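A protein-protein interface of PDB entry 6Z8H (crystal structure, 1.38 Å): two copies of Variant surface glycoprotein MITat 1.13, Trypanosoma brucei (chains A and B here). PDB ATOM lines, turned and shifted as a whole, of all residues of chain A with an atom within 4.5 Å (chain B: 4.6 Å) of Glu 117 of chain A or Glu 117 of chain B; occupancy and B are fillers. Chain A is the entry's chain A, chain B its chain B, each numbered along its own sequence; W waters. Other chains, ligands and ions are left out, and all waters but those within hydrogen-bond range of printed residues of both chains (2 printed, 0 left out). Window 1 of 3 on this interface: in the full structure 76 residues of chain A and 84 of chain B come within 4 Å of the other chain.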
ATOM      1  N   LEU A  42     -13.225  26.708 -23.690  1.00  0.00           N
ATOM      2  CA  LEU A  42     -13.584  25.734 -22.668  1.00  0.00           C
ATOM      3  C   LEU A  42     -14.128  24.455 -23.295  1.00  0.00           C
ATOM      4  O   LEU A  42     -13.904  23.364 -22.760  1.00  0.00           O
ATOM      5  CB  LEU A  42     -14.617  26.327 -21.719  1.00  0.00           C
ATOM      6  CG  LEU A  42     -14.115  27.401 -20.779  1.00  0.00           C
ATOM      7  CD1 LEU A  42     -15.282  28.038 -20.027  1.00  0.00           C
ATOM      8  CD2 LEU A  42     -13.133  26.837 -19.767  1.00  0.00           C
ATOM      9  N   ILE A 113      -5.268  23.150 -18.408  1.00  0.00           N
ATOM     10  CA  ILE A 113      -6.362  23.630 -17.570  1.00  0.00           C
ATOM     11  C   ILE A 113      -6.018  24.995 -16.987  1.00  0.00           C
ATOM     12  O   ILE A 113      -6.819  25.945 -17.031  1.00  0.00           O
ATOM     13  CB  ILE A 113      -6.672  22.639 -16.438  1.00  0.00           C
ATOM     14  CG1 ILE A 113      -7.289  21.356 -17.008  1.00  0.00           C
ATOM     15  CG2 ILE A 113      -7.556  23.323 -15.385  1.00  0.00           C
ATOM     16  CD1 ILE A 113      -7.320  20.213 -15.995  1.00  0.00           C
ATOM     17  N   SER A 114      -4.809  25.132 -16.446  1.00  0.00           N
ATOM     18  CA  SER A 114      -4.482  26.389 -15.784  1.00  0.00           C
ATOM     19  C   SER A 114      -4.401  27.531 -16.785  1.00  0.00           C
ATOM     20  O   SER A 114      -4.861  28.641 -16.501  1.00  0.00           O
ATOM     21  CB  SER A 114      -3.179  26.270 -15.017  1.00  0.00           C
ATOM     22  OG  SER A 114      -2.068  26.216 -15.869  1.00  0.00           O
ATOM     23  N   LYS A 115      -3.834  27.285 -17.966  1.00  0.00           N
ATOM     24  CA  LYS A 115      -3.661  28.350 -18.951  1.00  0.00           C
ATOM     25  C   LYS A 115      -4.980  28.731 -19.614  1.00  0.00           C
ATOM     26  O   LYS A 115      -5.254  29.919 -19.819  1.00  0.00           O
ATOM     27  CB  LYS A 115      -2.586  27.911 -19.944  1.00  0.00           C
ATOM     28  CG  LYS A 115      -1.187  27.984 -19.354  1.00  0.00           C
ATOM     29  CD  LYS A 115      -0.161  27.267 -20.200  1.00  0.00           C
ATOM     30  CE  LYS A 115       1.251  27.473 -19.674  1.00  0.00           C
ATOM     31  NZ  LYS A 115       2.255  27.172 -20.728  1.00  0.00           N
ATOM     32  N   ILE A 116      -5.847  27.764 -19.891  1.00  0.00           N
ATOM     33  CA  ILE A 116      -7.152  28.060 -20.476  1.00  0.00           C
ATOM     34  C   ILE A 116      -8.042  28.785 -19.480  1.00  0.00           C
ATOM     35  O   ILE A 116      -8.752  29.721 -19.858  1.00  0.00           O
ATOM     36  CB  ILE A 116      -7.816  26.778 -21.012  1.00  0.00           C
ATOM     37  CG1 ILE A 116      -7.234  26.379 -22.367  1.00  0.00           C
ATOM     38  CG2 ILE A 116      -9.327  26.952 -21.062  1.00  0.00           C
ATOM     39  CD1 ILE A 116      -7.745  25.085 -22.898  1.00  0.00           C
ATOM     40  N   GLU A 117      -8.051  28.367 -18.213  1.00  0.00           N
ATOM     41  CA  GLU A 117      -8.901  29.022 -17.223  1.00  0.00           C
ATOM     42  C   GLU A 117      -8.436  30.455 -16.941  1.00  0.00           C
ATOM     43  O   GLU A 117      -9.273  31.349 -16.771  1.00  0.00           O
ATOM     44  CB  GLU A 117      -8.974  28.186 -15.937  1.00  0.00           C
ATOM     45  CG  GLU A 117      -9.748  26.874 -16.113  1.00  0.00           C
ATOM     46  CD  GLU A 117     -11.266  27.065 -16.279  1.00  0.00           C
ATOM     47  OE1 GLU A 117     -11.735  28.215 -16.432  1.00  0.00           O
ATOM     48  OE2 GLU A 117     -11.968  26.024 -16.251  1.00  0.00           O
ATOM     49  N   GLU A 118      -7.117  30.717 -16.958  1.00  0.00           N
ATOM     50  CA  GLU A 118      -6.638  32.091 -16.836  1.00  0.00           C
ATOM     51  C   GLU A 118      -7.123  32.937 -18.006  1.00  0.00           C
ATOM     52  O   GLU A 118      -7.580  34.069 -17.810  1.00  0.00           O
ATOM     53  CB  GLU A 118      -5.108  32.126 -16.730  1.00  0.00           C
ATOM     54  CG  GLU A 118      -4.575  33.539 -16.513  1.00  0.00           C
ATOM     55  CD  GLU A 118      -3.095  33.615 -16.248  1.00  0.00           C
ATOM     56  OE1 GLU A 118      -2.485  32.572 -15.967  1.00  0.00           O
ATOM     57  OE2 GLU A 118      -2.505  34.705 -16.287  1.00  0.00           O
ATOM     58  N   ALA A 119      -7.033  32.417 -19.233  1.00  0.00           N
ATOM     59  CA  ALA A 119      -7.518  33.173 -20.385  1.00  0.00           C
ATOM     60  C   ALA A 119      -9.018  33.395 -20.313  1.00  0.00           C
ATOM     61  O   ALA A 119      -9.499  34.470 -20.687  1.00  0.00           O
ATOM     62  CB  ALA A 119      -7.132  32.445 -21.670  1.00  0.00           C
ATOM     63  N   ALA A 120      -9.758  32.430 -19.770  1.00  0.00           N
ATOM     64  CA  ALA A 120     -11.203  32.546 -19.617  1.00  0.00           C
ATOM     65  C   ALA A 120     -11.553  33.670 -18.662  1.00  0.00           C
ATOM     66  O   ALA A 120     -12.512  34.415 -18.900  1.00  0.00           O
ATOM     67  CB  ALA A 120     -11.767  31.214 -19.104  1.00  0.00           C
ATOM     68  N   GLY A 121     -10.755  33.850 -17.616  1.00  0.00           N
ATOM     69  CA  GLY A 121     -10.970  34.981 -16.728  1.00  0.00           C
ATOM     70  C   GLY A 121     -10.785  36.309 -17.447  1.00  0.00           C
ATOM     71  O   GLY A 121     -11.564  37.262 -17.262  1.00  0.00           O
ATOM     72  N   LEU B  42      -2.756  32.167  -5.841  1.00  0.00           N
ATOM     73  CA  LEU B  42      -2.008  31.061  -6.433  1.00  0.00           C
ATOM     74  C   LEU B  42      -1.152  30.353  -5.394  1.00  0.00           C
ATOM     75  O   LEU B  42      -1.041  29.127  -5.424  1.00  0.00           O
ATOM     76  CB  LEU B  42      -1.174  31.559  -7.606  1.00  0.00           C
ATOM     77  CG  LEU B  42      -2.002  32.061  -8.798  1.00  0.00           C
ATOM     78  CD1 LEU B  42      -1.080  32.678  -9.819  1.00  0.00           C
ATOM     79  CD2 LEU B  42      -2.771  30.889  -9.382  1.00  0.00           C
ATOM     80  N   ILE B 113      -8.814  24.474  -8.750  1.00  0.00           N
ATOM     81  CA  ILE B 113      -7.839  24.935  -9.720  1.00  0.00           C
ATOM     82  C   ILE B 113      -8.547  25.779 -10.755  1.00  0.00           C
ATOM     83  O   ILE B 113      -8.111  26.885 -11.087  1.00  0.00           O
ATOM     84  CB  ILE B 113      -7.141  23.741 -10.392  1.00  0.00           C
ATOM     85  CG1 ILE B 113      -6.175  23.025  -9.437  1.00  0.00           C
ATOM     86  CG2 ILE B 113      -6.409  24.251 -11.623  1.00  0.00           C
ATOM     87  CD1 ILE B 113      -5.753  21.652  -9.901  1.00  0.00           C
ATOM     88  N   SER B 114      -9.686  25.284 -11.248  1.00  0.00           N
ATOM     89  CA  SER B 114     -10.430  25.999 -12.284  1.00  0.00           C
ATOM     90  C   SER B 114     -10.893  27.366 -11.799  1.00  0.00           C
ATOM     91  O   SER B 114     -10.853  28.363 -12.545  1.00  0.00           O
ATOM     92  CB  SER B 114     -11.649  25.177 -12.681  1.00  0.00           C
ATOM     93  OG  SER B 114     -11.260  24.005 -13.348  1.00  0.00           O
ATOM     94  N   LYS B 115     -11.407  27.414 -10.580  1.00  0.00           N
ATOM     95  CA  LYS B 115     -11.960  28.662 -10.063  1.00  0.00           C
ATOM     96  C   LYS B 115     -10.867  29.662  -9.711  1.00  0.00           C
ATOM     97  O   LYS B 115     -11.009  30.862  -9.974  1.00  0.00           O
ATOM     98  CB  LYS B 115     -12.878  28.344  -8.881  1.00  0.00           C
ATOM     99  CG  LYS B 115     -14.145  27.669  -9.329  1.00  0.00           C
ATOM    100  CD  LYS B 115     -14.998  27.137  -8.233  1.00  0.00           C
ATOM    101  CE  LYS B 115     -16.306  26.596  -8.789  1.00  0.00           C
ATOM    102  NZ  LYS B 115     -17.278  26.263  -7.697  1.00  0.00           N
ATOM    103  N   ILE B 116      -9.769  29.210  -9.140  1.00  0.00           N
ATOM    104  CA  ILE B 116      -8.644  30.094  -8.790  1.00  0.00           C
ATOM    105  C   ILE B 116      -8.059  30.654 -10.082  1.00  0.00           C
ATOM    106  O   ILE B 116      -7.796  31.824 -10.118  1.00  0.00           O
ATOM    107  CB  ILE B 116      -7.571  29.343  -7.973  1.00  0.00           C
ATOM    108  CG1 ILE B 116      -8.110  28.901  -6.609  1.00  0.00           C
ATOM    109  CG2 ILE B 116      -6.258  30.088  -7.942  1.00  0.00           C
ATOM    110  CD1 ILE B 116      -7.861  29.616  -5.400  1.00  0.00           C
ATOM    111  N   GLU B 117      -7.882  29.835 -11.113  1.00  0.00           N
ATOM    112  CA  GLU B 117      -7.213  30.295 -12.320  1.00  0.00           C
ATOM    113  C   GLU B 117      -8.105  31.280 -13.067  1.00  0.00           C
ATOM    114  O   GLU B 117      -7.601  32.249 -13.631  1.00  0.00           O
ATOM    115  CB  GLU B 117      -6.764  29.111 -13.176  1.00  0.00           C
ATOM    116  CG  GLU B 117      -5.640  28.326 -12.531  1.00  0.00           C
ATOM    117  CD  GLU B 117      -4.274  28.985 -12.633  1.00  0.00           C
ATOM    118  OE1 GLU B 117      -4.201  30.153 -13.092  1.00  0.00           O
ATOM    119  OE2 GLU B 117      -3.278  28.315 -12.243  1.00  0.00           O
ATOM    120  N   GLU B 118      -9.433  31.052 -13.091  1.00  0.00           N
ATOM    121  CA  GLU B 118     -10.341  32.040 -13.688  1.00  0.00           C
ATOM    122  C   GLU B 118     -10.251  33.373 -12.937  1.00  0.00           C
ATOM    123  O   GLU B 118     -10.204  34.448 -13.552  1.00  0.00           O
ATOM    124  CB  GLU B 118     -11.774  31.501 -13.690  1.00  0.00           C
ATOM    125  CG  GLU B 118     -12.777  32.485 -14.313  1.00  0.00           C
ATOM    126  CD  GLU B 118     -14.175  31.914 -14.480  1.00  0.00           C
ATOM    127  OE1 GLU B 118     -14.383  30.716 -14.329  1.00  0.00           O
ATOM    128  OE2 GLU B 118     -15.108  32.649 -14.818  1.00  0.00           O
ATOM    129  N   ALA B 119     -10.249  33.333 -11.608  1.00  0.00           N
ATOM    130  CA  ALA B 119     -10.091  34.577 -10.854  1.00  0.00           C
ATOM    131  C   ALA B 119      -8.764  35.262 -11.170  1.00  0.00           C
ATOM    132  O   ALA B 119      -8.710  36.485 -11.307  1.00  0.00           O
ATOM    133  CB  ALA B 119     -10.257  34.330  -9.359  1.00  0.00           C
ATOM    134  N   ALA B 120      -7.679  34.499 -11.245  1.00  0.00           N
ATOM    135  CA  ALA B 120      -6.367  35.039 -11.583  1.00  0.00           C
ATOM    136  C   ALA B 120      -6.403  35.774 -12.916  1.00  0.00           C
ATOM    137  O   ALA B 120      -5.801  36.840 -13.056  1.00  0.00           O
ATOM    138  CB  ALA B 120      -5.329  33.894 -11.572  1.00  0.00           C
ATOM    139  N   GLY B 121      -7.112  35.225 -13.897  1.00  0.00           N
ATOM    140  CA  GLY B 121      -7.264  35.930 -15.163  1.00  0.00           C
ATOM    141  C   GLY B 121      -7.944  37.282 -15.002  1.00  0.00           C
ATOM    142  O   GLY B 121      -7.522  38.283 -15.597  1.00  0.00           O
HETATM  143  O   HOH W   1      -2.366  32.285 -13.186  1.00  0.00           O
HETATM  144  O   HOH W   2     -14.418  29.092 -16.797  1.00  0.00           O
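Among the printed residues, merely in contact across the chains: Ser 114 of chain A with Glu 117 of chain B (3.4 Å), Glu 117 of chain A with Ser 114 of chain B (3.6 Å), Glu 117 of chain A with Glu 117 of chain B (3.7 Å), Glu 117 of chain A with Glu 118 of chain B (3.3 Å), Glu 118 of chain A with Glu 117 of chain B (3.4 Å), Glu 118 of chain A with Gly 121 of chain B (3.3 Å), Gly 121 of chain A with Glu 118 of chain B (3.3 Å) and Gly 121 of chain A with Gly 121 of chain B (3.9 Å).
Of the printed residues of chain B, Ser 114 of chain A touches Glu 117 (3.4 Å). Lys 115 of chain A touches none of the printed residues of chain B. Of chain B, only Ser 114, Glu 117 and Glu 118 come within 4 Å of Glu 117 of chain A. Of the printed residues of chain B, Glu 118 of chain A touches Glu 117 and Gly 121. Printed residues of chain B within 4 Å of Gly 121 of chain A: Glu 118 (3.3 Å) and Gly 121 (3.9 Å). Leu 42 of chain B touches none of the printed residues of chain A. Of the printed residues of chain A, Ser 114 of chain B touches Glu 117. Glu 117 of chain B touches just these residues of chain A: Ser 114, Glu 117 and Glu 118. Of the printed residues of chain A, Gly 121 of chain B touches Glu 118 (3.3 Å) and Gly 121 (3.9 Å). The nearest printed residue of chain B that does not touch Glu 117 of chain A is Ile 113 of chain B (5.1 Å). The nearest printed residue of chain A that does not touch Glu 117 of chain B is Ile 113 of chain A (5.0 Å).
Of the 10 printed residues of chain A, 4 touch a printed residue of chain B. Printed residues of chain A that touch a printed residue of chain B: Ser 114, Glu 117, Glu 118 and Gly 121. Of the 10 printed residues of chain B, 4 touch a printed residue of chain A. Printed residues of chain B that touch a printed residue of chain A: Ser 114, Glu 117, Glu 118 and Gly 121. Among the printed residues, 8 pairs touch across the chains.
Ser 114 of chain A touches Glu 117 of chain B, and with the chains exchanged Glu 117 of chain A touches Ser 114 of chain B. Glu 117 of chain B touches its own counterpart, Glu 117 of chain A. Glu 118 of chain A touches Gly 121 of chain B, and with the chains exchanged Gly 121 of chain A touches Glu 118 of chain B. Gly 121 of chain A touches its own counterpart, Gly 121 of chain B. Positions printed for both chains: 42, 113, 114, 115, 116, 117, 118, 119, 120 and 121.
Water W1 bridges the side-chain carboxylate (OE1) of Glu 118 of chain A (2.8 Å) and the side-chain carboxylate (OE1) of Glu 117 of chain B (2.8 Å). Water W2 bridges OE1 of Glu 117 of chain A (2.8 Å) and OE1 of Glu 118 of chain B (3.0 Å).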
